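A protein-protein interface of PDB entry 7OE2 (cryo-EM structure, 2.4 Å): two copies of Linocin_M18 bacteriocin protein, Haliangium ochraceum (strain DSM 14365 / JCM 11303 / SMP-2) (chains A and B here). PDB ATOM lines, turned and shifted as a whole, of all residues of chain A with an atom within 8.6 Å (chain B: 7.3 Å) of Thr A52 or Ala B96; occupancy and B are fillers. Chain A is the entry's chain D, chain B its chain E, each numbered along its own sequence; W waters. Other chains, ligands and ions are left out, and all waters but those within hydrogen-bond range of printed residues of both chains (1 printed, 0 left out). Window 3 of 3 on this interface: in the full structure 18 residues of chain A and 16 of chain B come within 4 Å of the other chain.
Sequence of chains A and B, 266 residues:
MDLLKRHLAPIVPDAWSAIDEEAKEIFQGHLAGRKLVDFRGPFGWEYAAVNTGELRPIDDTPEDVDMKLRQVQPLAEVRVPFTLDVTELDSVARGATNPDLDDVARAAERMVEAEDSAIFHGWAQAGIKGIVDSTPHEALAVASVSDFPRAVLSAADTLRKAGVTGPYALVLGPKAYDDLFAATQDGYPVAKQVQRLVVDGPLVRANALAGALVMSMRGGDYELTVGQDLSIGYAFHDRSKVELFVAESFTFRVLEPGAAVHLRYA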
ATOM      1  N   ARG A  40       7.613 -24.187 -17.205  1.00  0.00           N
ATOM      2  CA  ARG A  40       7.993 -22.785 -17.124  1.00  0.00           C
ATOM      3  C   ARG A  40       6.713 -21.979 -16.967  1.00  0.00           C
ATOM      4  O   ARG A  40       5.894 -21.892 -17.895  1.00  0.00           O
ATOM      5  CB  ARG A  40       8.812 -22.362 -18.336  1.00  0.00           C
ATOM      6  CG  ARG A  40      10.286 -22.632 -18.139  1.00  0.00           C
ATOM      7  CD  ARG A  40      11.129 -22.065 -19.257  1.00  0.00           C
ATOM      8  NE  ARG A  40      11.347 -20.632 -19.105  1.00  0.00           N
ATOM      9  CZ  ARG A  40      11.022 -19.732 -20.023  1.00  0.00           C
ATOM     10  NH1 ARG A  40      10.469 -20.118 -21.161  1.00  0.00           N
ATOM     11  NH2 ARG A  40      11.255 -18.448 -19.802  1.00  0.00           N
ATOM     12  N   TYR A  47       3.823 -12.720 -23.210  1.00  0.00           N
ATOM     13  CA  TYR A  47       4.927 -13.611 -23.538  1.00  0.00           C
ATOM     14  C   TYR A  47       4.717 -14.216 -24.918  1.00  0.00           C
ATOM     15  O   TYR A  47       3.703 -14.869 -25.168  1.00  0.00           O
ATOM     16  CB  TYR A  47       5.027 -14.693 -22.476  1.00  0.00           C
ATOM     17  CG  TYR A  47       6.334 -15.431 -22.428  1.00  0.00           C
ATOM     18  CD1 TYR A  47       7.407 -14.936 -21.703  1.00  0.00           C
ATOM     19  CD2 TYR A  47       6.489 -16.635 -23.090  1.00  0.00           C
ATOM     20  CE1 TYR A  47       8.593 -15.620 -21.649  1.00  0.00           C
ATOM     21  CE2 TYR A  47       7.667 -17.317 -23.044  1.00  0.00           C
ATOM     22  CZ  TYR A  47       8.715 -16.811 -22.322  1.00  0.00           C
ATOM     23  OH  TYR A  47       9.893 -17.504 -22.281  1.00  0.00           O
ATOM     24  N   ALA A  49       7.603 -15.658 -27.137  1.00  0.00           N
ATOM     25  CA  ALA A  49       8.520 -16.677 -27.616  1.00  0.00           C
ATOM     26  C   ALA A  49       9.466 -17.077 -26.501  1.00  0.00           C
ATOM     27  O   ALA A  49       9.713 -16.313 -25.570  1.00  0.00           O
ATOM     28  CB  ALA A  49       9.307 -16.204 -28.840  1.00  0.00           C
ATOM     29  N   VAL A  50       9.973 -18.292 -26.601  1.00  0.00           N
ATOM     30  CA  VAL A  50      10.990 -18.802 -25.693  1.00  0.00           C
ATOM     31  C   VAL A  50      12.354 -18.537 -26.303  1.00  0.00           C
ATOM     32  O   VAL A  50      12.604 -18.889 -27.458  1.00  0.00           O
ATOM     33  CB  VAL A  50      10.789 -20.304 -25.426  1.00  0.00           C
ATOM     34  CG1 VAL A  50      11.963 -20.863 -24.639  1.00  0.00           C
ATOM     35  CG2 VAL A  50       9.504 -20.536 -24.690  1.00  0.00           C
ATOM     36  N   ASN A  51      13.229 -17.903 -25.534  1.00  0.00           N
ATOM     37  CA  ASN A  51      14.614 -17.709 -25.934  1.00  0.00           C
ATOM     38  C   ASN A  51      15.377 -19.022 -25.775  1.00  0.00           C
ATOM     39  O   ASN A  51      15.471 -19.559 -24.670  1.00  0.00           O
ATOM     40  CB  ASN A  51      15.243 -16.597 -25.098  1.00  0.00           C
ATOM     41  CG  ASN A  51      16.754 -16.616 -25.132  1.00  0.00           C
ATOM     42  OD1 ASN A  51      17.358 -16.668 -26.193  1.00  0.00           O
ATOM     43  ND2 ASN A  51      17.369 -16.573 -23.964  1.00  0.00           N
ATOM     44  N   THR A  52      15.904 -19.543 -26.877  1.00  0.00           N
ATOM     45  CA  THR A  52      16.682 -20.772 -26.843  1.00  0.00           C
ATOM     46  C   THR A  52      18.157 -20.539 -26.543  1.00  0.00           C
ATOM     47  O   THR A  52      18.870 -21.500 -26.251  1.00  0.00           O
ATOM     48  CB  THR A  52      16.548 -21.535 -28.167  1.00  0.00           C
ATOM     49  OG1 THR A  52      17.320 -20.890 -29.183  1.00  0.00           O
ATOM     50  CG2 THR A  52      15.098 -21.611 -28.608  1.00  0.00           C
ATOM     51  N   GLY A  53      18.623 -19.296 -26.599  1.00  0.00           N
ATOM     52  CA  GLY A  53      20.010 -18.967 -26.391  1.00  0.00           C
ATOM     53  C   GLY A  53      20.919 -19.263 -27.558  1.00  0.00           C
ATOM     54  O   GLY A  53      22.123 -19.040 -27.448  1.00  0.00           O
ATOM     55  N   GLU A  54      20.387 -19.741 -28.672  1.00  0.00           N
ATOM     56  CA  GLU A  54      21.187 -20.152 -29.813  1.00  0.00           C
ATOM     57  C   GLU A  54      21.268 -19.054 -30.868  1.00  0.00           C
ATOM     58  O   GLU A  54      20.461 -18.126 -30.907  1.00  0.00           O
ATOM     59  CB  GLU A  54      20.617 -21.428 -30.428  1.00  0.00           C
ATOM     60  CG  GLU A  54      20.908 -22.667 -29.606  1.00  0.00           C
ATOM     61  CD  GLU A  54      19.705 -23.569 -29.445  1.00  0.00           C
ATOM     62  OE1 GLU A  54      19.204 -23.695 -28.309  1.00  0.00           O
ATOM     63  OE2 GLU A  54      19.259 -24.158 -30.451  1.00  0.00           O
ATOM     64  N   LEU A  55      22.271 -19.183 -31.727  1.00  0.00           N
ATOM     65  CA  LEU A  55      22.525 -18.252 -32.812  1.00  0.00           C
ATOM     66  C   LEU A  55      22.605 -19.020 -34.118  1.00  0.00           C
ATOM     67  O   LEU A  55      23.057 -20.163 -34.154  1.00  0.00           O
ATOM     68  CB  LEU A  55      23.822 -17.476 -32.597  1.00  0.00           C
ATOM     69  CG  LEU A  55      23.796 -16.322 -31.606  1.00  0.00           C
ATOM     70  CD1 LEU A  55      25.198 -15.857 -31.312  1.00  0.00           C
ATOM     71  CD2 LEU A  55      22.976 -15.191 -32.164  1.00  0.00           C
ATOM     72  N   ARG A  56      22.156 -18.387 -35.192  1.00  0.00           N
ATOM     73  CA  ARG A  56      22.201 -18.984 -36.508  1.00  0.00           C
ATOM     74  C   ARG A  56      23.022 -18.103 -37.436  1.00  0.00           C
ATOM     75  O   ARG A  56      22.791 -16.888 -37.491  1.00  0.00           O
ATOM     76  CB  ARG A  56      20.796 -19.172 -37.084  1.00  0.00           C
ATOM     77  CG  ARG A  56      20.785 -19.926 -38.396  1.00  0.00           C
ATOM     78  CD  ARG A  56      19.521 -19.679 -39.212  1.00  0.00           C
ATOM     79  NE  ARG A  56      18.810 -18.465 -38.818  1.00  0.00           N
ATOM     80  CZ  ARG A  56      17.564 -18.445 -38.360  1.00  0.00           C
ATOM     81  NH1 ARG A  56      16.881 -19.573 -38.245  1.00  0.00           N
ATOM     82  NH2 ARG A  56      16.997 -17.298 -38.022  1.00  0.00           N
ATOM     83  N   LEU A  69      21.864 -14.457 -36.188  1.00  0.00           N
ATOM     84  CA  LEU A  69      20.479 -14.205 -35.814  1.00  0.00           C
ATOM     85  C   LEU A  69      20.104 -15.022 -34.588  1.00  0.00           C
ATOM     86  O   LEU A  69      20.385 -16.219 -34.528  1.00  0.00           O
ATOM     87  CB  LEU A  69      19.550 -14.538 -36.980  1.00  0.00           C
ATOM     88  CG  LEU A  69      18.392 -13.586 -37.254  1.00  0.00           C
ATOM     89  CD1 LEU A  69      18.870 -12.163 -37.394  1.00  0.00           C
ATOM     90  CD2 LEU A  69      17.693 -14.031 -38.514  1.00  0.00           C
ATOM     91  N   ARG A  70      19.473 -14.374 -33.615  1.00  0.00           N
ATOM     92  CA  ARG A  70      18.971 -15.080 -32.445  1.00  0.00           C
ATOM     93  C   ARG A  70      17.857 -16.049 -32.832  1.00  0.00           C
ATOM     94  O   ARG A  70      17.093 -15.813 -33.768  1.00  0.00           O
ATOM     95  CB  ARG A  70      18.458 -14.094 -31.403  1.00  0.00           C
ATOM     96  CG  ARG A  70      19.527 -13.326 -30.657  1.00  0.00           C
ATOM     97  CD  ARG A  70      20.463 -14.225 -29.870  1.00  0.00           C
ATOM     98  NE  ARG A  70      19.884 -14.680 -28.615  1.00  0.00           N
ATOM     99  CZ  ARG A  70      20.169 -14.171 -27.427  1.00  0.00           C
ATOM    100  NH1 ARG A  70      21.033 -13.185 -27.317  1.00  0.00           N
ATOM    101  NH2 ARG A  70      19.589 -14.656 -26.349  1.00  0.00           N
ATOM    102  N   GLN A  71      17.787 -17.162 -32.115  1.00  0.00           N
ATOM    103  CA  GLN A  71      16.765 -18.178 -32.323  1.00  0.00           C
ATOM    104  C   GLN A  71      15.772 -18.142 -31.174  1.00  0.00           C
ATOM    105  O   GLN A  71      16.164 -18.071 -30.009  1.00  0.00           O
ATOM    106  CB  GLN A  71      17.379 -19.569 -32.435  1.00  0.00           C
ATOM    107  CG  GLN A  71      18.486 -19.684 -33.450  1.00  0.00           C
ATOM    108  CD  GLN A  71      17.998 -19.473 -34.859  1.00  0.00           C
ATOM    109  OE1 GLN A  71      18.172 -18.403 -35.431  1.00  0.00           O
ATOM    110  NE2 GLN A  71      17.378 -20.492 -35.429  1.00  0.00           N
ATOM    111  N   VAL A  72      14.487 -18.169 -31.509  1.00  0.00           N
ATOM    112  CA  VAL A  72      13.423 -18.250 -30.524  1.00  0.00           C
ATOM    113  C   VAL A  72      12.445 -19.322 -30.971  1.00  0.00           C
ATOM    114  O   VAL A  72      12.443 -19.759 -32.121  1.00  0.00           O
ATOM    115  CB  VAL A  72      12.684 -16.906 -30.320  1.00  0.00           C
ATOM    116  CG1 VAL A  72      13.539 -15.931 -29.541  1.00  0.00           C
ATOM    117  CG2 VAL A  72      12.255 -16.322 -31.652  1.00  0.00           C
ATOM    118  N   GLN A  73      11.618 -19.756 -30.038  1.00  0.00           N
ATOM    119  CA  GLN A  73      10.476 -20.604 -30.362  1.00  0.00           C
ATOM    120  C   GLN A  73       9.196 -19.875 -29.997  1.00  0.00           C
ATOM    121  O   GLN A  73       8.885 -19.743 -28.802  1.00  0.00           O
ATOM    122  CB  GLN A  73      10.553 -21.947 -29.643  1.00  0.00           C
ATOM    123  CG  GLN A  73       9.623 -22.965 -30.247  1.00  0.00           C
ATOM    124  CD  GLN A  73       9.903 -24.356 -29.782  1.00  0.00           C
ATOM    125  OE1 GLN A  73       9.228 -24.871 -28.902  1.00  0.00           O
ATOM    126  NE2 GLN A  73      10.906 -24.981 -30.370  1.00  0.00           N
ATOM    127  N   PRO A  74       8.445 -19.358 -30.964  1.00  0.00           N
ATOM    128  CA  PRO A  74       7.206 -18.643 -30.636  1.00  0.00           C
ATOM    129  C   PRO A  74       6.138 -19.557 -30.057  1.00  0.00           C
ATOM    130  O   PRO A  74       6.037 -20.736 -30.394  1.00  0.00           O
ATOM    131  CB  PRO A  74       6.763 -18.056 -31.978  1.00  0.00           C
ATOM    132  CG  PRO A  74       7.536 -18.757 -33.000  1.00  0.00           C
ATOM    133  CD  PRO A  74       8.765 -19.305 -32.396  1.00  0.00           C
ATOM    134  N   GLU A 223      10.685 -29.314 -21.660  1.00  0.00           N
ATOM    135  CA  GLU A 223      10.270 -28.064 -21.048  1.00  0.00           C
ATOM    136  C   GLU A 223       9.020 -27.548 -21.739  1.00  0.00           C
ATOM    137  O   GLU A 223       9.045 -27.236 -22.927  1.00  0.00           O
ATOM    138  CB  GLU A 223      11.416 -27.053 -21.106  1.00  0.00           C
ATOM    139  CG  GLU A 223      11.098 -25.654 -20.669  1.00  0.00           C
ATOM    140  CD  GLU A 223      12.260 -24.711 -20.942  1.00  0.00           C
ATOM    141  OE1 GLU A 223      13.190 -24.666 -20.109  1.00  0.00           O
ATOM    142  OE2 GLU A 223      12.255 -24.031 -21.993  1.00  0.00           O
ATOM    143  N   THR A 251       4.261 -23.376 -25.569  1.00  0.00           N
ATOM    144  CA  THR A 251       5.100 -24.115 -26.498  1.00  0.00           C
ATOM    145  C   THR A 251       5.837 -25.194 -25.719  1.00  0.00           C
ATOM    146  O   THR A 251       5.943 -25.142 -24.496  1.00  0.00           O
ATOM    147  CB  THR A 251       6.056 -23.183 -27.271  1.00  0.00           C
ATOM    148  OG1 THR A 251       6.554 -23.860 -28.426  1.00  0.00           O
ATOM    149  CG2 THR A 251       7.206 -22.717 -26.413  1.00  0.00           C
ATOM    150  N   ARG A 253       9.409 -27.639 -25.710  1.00  0.00           N
ATOM    151  CA  ARG A 253      10.763 -27.832 -26.199  1.00  0.00           C
ATOM    152  C   ARG A 253      11.322 -29.156 -25.708  1.00  0.00           C
ATOM    153  O   ARG A 253      11.172 -29.514 -24.536  1.00  0.00           O
ATOM    154  CB  ARG A 253      11.688 -26.700 -25.748  1.00  0.00           C
ATOM    155  CG  ARG A 253      11.376 -25.362 -26.361  1.00  0.00           C
ATOM    156  CD  ARG A 253      12.267 -24.295 -25.806  1.00  0.00           C
ATOM    157  NE  ARG A 253      13.629 -24.440 -26.294  1.00  0.00           N
ATOM    158  CZ  ARG A 253      14.710 -24.171 -25.578  1.00  0.00           C
ATOM    159  NH1 ARG A 253      14.594 -23.734 -24.337  1.00  0.00           N
ATOM    160  NH2 ARG A 253      15.905 -24.342 -26.111  1.00  0.00           N
ATOM    161  N   LEU A 255      14.763 -30.427 -24.941  1.00  0.00           N
ATOM    162  CA  LEU A 255      16.140 -29.989 -24.750  1.00  0.00           C
ATOM    163  C   LEU A 255      17.126 -31.132 -24.952  1.00  0.00           C
ATOM    164  O   LEU A 255      18.194 -30.932 -25.535  1.00  0.00           O
ATOM    165  CB  LEU A 255      16.299 -29.373 -23.366  1.00  0.00           C
ATOM    166  CG  LEU A 255      15.180 -28.395 -23.018  1.00  0.00           C
ATOM    167  CD1 LEU A 255      15.051 -28.202 -21.525  1.00  0.00           C
ATOM    168  CD2 LEU A 255      15.414 -27.074 -23.717  1.00  0.00           C
ATOM    169  N   ALA B  18      27.607 -25.572 -15.574  1.00  0.00           N
ATOM    170  CA  ALA B  18      26.964 -26.591 -16.399  1.00  0.00           C
ATOM    171  C   ALA B  18      27.875 -27.797 -16.614  1.00  0.00           C
ATOM    172  O   ALA B  18      27.425 -28.944 -16.518  1.00  0.00           O
ATOM    173  CB  ALA B  18      26.529 -25.994 -17.735  1.00  0.00           C
ATOM    174  N   GLU B  88      29.373 -23.150 -28.135  1.00  0.00           N
ATOM    175  CA  GLU B  88      28.385 -23.850 -27.328  1.00  0.00           C
ATOM    176  C   GLU B  88      28.433 -23.392 -25.879  1.00  0.00           C
ATOM    177  O   GLU B  88      27.394 -23.269 -25.225  1.00  0.00           O
ATOM    178  CB  GLU B  88      28.607 -25.357 -27.421  1.00  0.00           C
ATOM    179  CG  GLU B  88      28.205 -25.965 -28.745  1.00  0.00           C
ATOM    180  CD  GLU B  88      26.702 -26.038 -28.927  1.00  0.00           C
ATOM    181  OE1 GLU B  88      26.244 -26.020 -30.085  1.00  0.00           O
ATOM    182  OE2 GLU B  88      25.974 -26.121 -27.917  1.00  0.00           O
ATOM    183  N   LEU B  89      29.629 -23.140 -25.357  1.00  0.00           N
ATOM    184  CA  LEU B  89      29.750 -22.678 -23.984  1.00  0.00           C
ATOM    185  C   LEU B  89      29.356 -21.216 -23.834  1.00  0.00           C
ATOM    186  O   LEU B  89      28.855 -20.826 -22.777  1.00  0.00           O
ATOM    187  CB  LEU B  89      31.172 -22.907 -23.480  1.00  0.00           C
ATOM    188  CG  LEU B  89      31.620 -24.368 -23.438  1.00  0.00           C
ATOM    189  CD1 LEU B  89      33.077 -24.461 -23.079  1.00  0.00           C
ATOM    190  CD2 LEU B  89      30.770 -25.179 -22.470  1.00  0.00           C
ATOM    191  N   ASP B  90      29.576 -20.395 -24.861  1.00  0.00           N
ATOM    192  CA  ASP B  90      29.087 -19.021 -24.829  1.00  0.00           C
ATOM    193  C   ASP B  90      27.567 -18.965 -24.879  1.00  0.00           C
ATOM    194  O   ASP B  90      26.972 -18.003 -24.388  1.00  0.00           O
ATOM    195  CB  ASP B  90      29.681 -18.211 -25.982  1.00  0.00           C
ATOM    196  CG  ASP B  90      31.196 -18.136 -25.934  1.00  0.00           C
ATOM    197  OD1 ASP B  90      31.810 -17.849 -26.981  1.00  0.00           O
ATOM    198  OD2 ASP B  90      31.779 -18.356 -24.853  1.00  0.00           O
ATOM    199  N   SER B  91      26.935 -19.985 -25.465  1.00  0.00           N
ATOM    200  CA  SER B  91      25.477 -20.039 -25.537  1.00  0.00           C
ATOM    201  C   SER B  91      24.822 -19.891 -24.171  1.00  0.00           C
ATOM    202  O   SER B  91      23.750 -19.292 -24.060  1.00  0.00           O
ATOM    203  CB  SER B  91      25.033 -21.347 -26.179  1.00  0.00           C
ATOM    204  OG  SER B  91      25.169 -21.296 -27.577  1.00  0.00           O
ATOM    205  N   VAL B  92      25.427 -20.445 -23.118  1.00  0.00           N
ATOM    206  CA  VAL B  92      24.770 -20.403 -21.819  1.00  0.00           C
ATOM    207  C   VAL B  92      24.762 -18.997 -21.237  1.00  0.00           C
ATOM    208  O   VAL B  92      23.894 -18.678 -20.420  1.00  0.00           O
ATOM    209  CB  VAL B  92      25.392 -21.427 -20.839  1.00  0.00           C
ATOM    210  CG1 VAL B  92      26.282 -22.404 -21.566  1.00  0.00           C
ATOM    211  CG2 VAL B  92      26.121 -20.755 -19.704  1.00  0.00           C
ATOM    212  N   ALA B  93      25.691 -18.134 -21.647  1.00  0.00           N
ATOM    213  CA  ALA B  93      25.618 -16.737 -21.247  1.00  0.00           C
ATOM    214  C   ALA B  93      24.510 -15.988 -21.976  1.00  0.00           C
ATOM    215  O   ALA B  93      24.063 -14.947 -21.493  1.00  0.00           O
ATOM    216  CB  ALA B  93      26.962 -16.052 -21.475  1.00  0.00           C
ATOM    217  N   ARG B  94      24.055 -16.495 -23.114  1.00  0.00           N
ATOM    218  CA  ARG B  94      22.904 -15.948 -23.811  1.00  0.00           C
ATOM    219  C   ARG B  94      21.593 -16.576 -23.364  1.00  0.00           C
ATOM    220  O   ARG B  94      20.550 -16.269 -23.939  1.00  0.00           O
ATOM    221  CB  ARG B  94      23.068 -16.119 -25.319  1.00  0.00           C
ATOM    222  CG  ARG B  94      24.009 -15.123 -25.917  1.00  0.00           C
ATOM    223  CD  ARG B  94      24.084 -15.250 -27.403  1.00  0.00           C
ATOM    224  NE  ARG B  94      25.327 -14.686 -27.901  1.00  0.00           N
ATOM    225  CZ  ARG B  94      26.443 -15.378 -28.082  1.00  0.00           C
ATOM    226  NH1 ARG B  94      26.478 -16.672 -27.811  1.00  0.00           N
ATOM    227  NH2 ARG B  94      27.524 -14.773 -28.538  1.00  0.00           N
ATOM    228  N   GLY B  95      21.624 -17.445 -22.360  1.00  0.00           N
ATOM    229  CA  GLY B  95      20.431 -18.039 -21.812  1.00  0.00           C
ATOM    230  C   GLY B  95      20.135 -19.449 -22.262  1.00  0.00           C
ATOM    231  O   GLY B  95      19.081 -19.976 -21.905  1.00  0.00           O
ATOM    232  N   ALA B  96      21.015 -20.073 -23.035  1.00  0.00           N
ATOM    233  CA  ALA B  96      20.802 -21.458 -23.423  1.00  0.00           C
ATOM    234  C   ALA B  96      20.960 -22.379 -22.221  1.00  0.00           C
ATOM    235  O   ALA B  96      21.873 -22.222 -21.409  1.00  0.00           O
ATOM    236  CB  ALA B  96      21.769 -21.863 -24.528  1.00  0.00           C
ATOM    237  N   THR B  97      20.053 -23.348 -22.110  1.00  0.00           N
ATOM    238  CA  THR B  97      20.051 -24.288 -21.001  1.00  0.00           C
ATOM    239  C   THR B  97      20.559 -25.669 -21.381  1.00  0.00           C
ATOM    240  O   THR B  97      20.806 -26.481 -20.487  1.00  0.00           O
ATOM    241  CB  THR B  97      18.641 -24.422 -20.406  1.00  0.00           C
ATOM    242  OG1 THR B  97      17.665 -24.382 -21.455  1.00  0.00           O
ATOM    243  CG2 THR B  97      18.374 -23.301 -19.422  1.00  0.00           C
ATOM    244  N   ASN B  98      20.745 -25.950 -22.666  1.00  0.00           N
ATOM    245  CA  ASN B  98      21.212 -27.260 -23.123  1.00  0.00           C
ATOM    246  C   ASN B  98      22.405 -27.117 -24.063  1.00  0.00           C
ATOM    247  O   ASN B  98      22.334 -27.483 -25.239  1.00  0.00           O
ATOM    248  CB  ASN B  98      20.067 -28.016 -23.794  1.00  0.00           C
ATOM    249  CG  ASN B  98      19.458 -27.250 -24.949  1.00  0.00           C
ATOM    250  OD1 ASN B  98      19.117 -26.085 -24.812  1.00  0.00           O
ATOM    251  ND2 ASN B  98      19.303 -27.909 -26.082  1.00  0.00           N
ATOM    252  N   PRO B  99      23.535 -26.617 -23.569  1.00  0.00           N
ATOM    253  CA  PRO B  99      24.747 -26.614 -24.392  1.00  0.00           C
ATOM    254  C   PRO B  99      25.215 -28.028 -24.692  1.00  0.00           C
ATOM    255  O   PRO B  99      24.993 -28.961 -23.920  1.00  0.00           O
ATOM    256  CB  PRO B  99      25.760 -25.865 -23.525  1.00  0.00           C
ATOM    257  CG  PRO B  99      25.271 -26.057 -22.142  1.00  0.00           C
ATOM    258  CD  PRO B  99      23.790 -26.042 -22.238  1.00  0.00           C
HETATM  259  O   HOH W   1      24.500 -18.598 -28.544  1.00  0.00           O
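ND2 of Asn A51 lies within hydrogen-bond range of O of Arg B94.
The guanidinium group (NH2) of Arg A70 lies within hydrogen-bond range of the backbone carbonyl oxygen (O) of Arg B94 (3.1 Å).
O of Leu A255 sits at hydrogen-bond distance from ND2 of Asn B98 (3.3 Å).
The side-chain amide oxygen (OD1) of Asn A51 is in hydrogen-bond range of the backbone NH (N) of Gly A53.
The guanidinium group (NH2) of Arg A70 sits at hydrogen-bond distance from the side-chain amide oxygen (OD1) of Asn A51 (3.0 Å).
The backbone NH of Glu A54 lies close to the side-chain hydroxyl of Thr A52 (3.3 Å).
OG1 of Thr A52 is in hydrogen-bond range of O of Gln A71, at 3.2 Å.
The side-chain carboxylate (OE2) of Glu A223 lies within salt-bridge range of the guanidinium group (NH1) of Arg A253 (3.3 Å).
The backbone NH (N) of Ala B96 lies within hydrogen-bond range of the backbone carbonyl oxygen (O) of Ser B91, at 3.0 Å.
Ala B96 touches Thr A52 (CB to O, 3.4 Å).
Ser B91 touches Gly A53 (O to O, 3.8 Å).
Gly A53 touches Arg B94.
Ala B96 touches Gly A53.
Leu A55 touches Arg B94 (CD1 to CZ, 3.5 Å).
Arg A253 touches Asn B98 (NH2 to OD1, 3.9 Å).
Thr A52 touches just one residue of chain B: Ala B96 (3.4 Å).
Of chain A, only Thr A52 (3.4 Å) and Gly A53 (3.7 Å) come within 4 Å of Ala B96.
No residue of chain A comes within 4 Å of Thr B97.
Printed residues of chain B within 4 Å of Leu A255: Asn B98 (3.3 Å).
Of the printed residues of chain A, Arg B94 touches Asn A51, Gly A53, Leu A55 and Arg A70.
Of the printed residues of chain B, Arg A70 touches Arg B94 (3.1 Å).
Printed residues of chain B within 4 Å of Asn A51: Arg B94 (3.2 Å).
Of the printed residues of chain B, Gly A53 touches Ser B91 (3.8 Å), Arg B94 (3.7 Å) and Ala B96 (3.7 Å).
The nearest residue of chain A that does not touch Ala B96 is Glu A54 (4.9 Å).
The nearest printed residue of chain B that does not touch Leu A255 is Thr B97 (4.2 Å).
Of the 20 printed residues of chain A, 7 touch a printed residue of chain B.
Printed residues of chain A that touch a printed residue of chain B: Asn A51, Thr A52, Gly A53, Leu A55, Arg A70, Arg A253 and Leu A255.
Along chain A the printed residues that touch a printed residue of chain B span positions 51 to 255.
Of the 13 printed residues of chain B, 4 touch a printed residue of chain A.
Printed residues of chain B that touch a printed residue of chain A: Ser B91, Arg B94, Ala B96 and Asn B98.
Along chain B the printed residues that touch a printed residue of chain A span positions 91 to 98.
No position is printed for both chains.
Of the 9 pairs that touch across the chains among the printed residues, none has its exchanged pair printed and touching as well.
Water W1 lies within hydrogen-bond range of the backbone carbonyl oxygen of Gly A53, the guanidinium group of Arg B94 and the side-chain hydroxyl of Ser B91.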
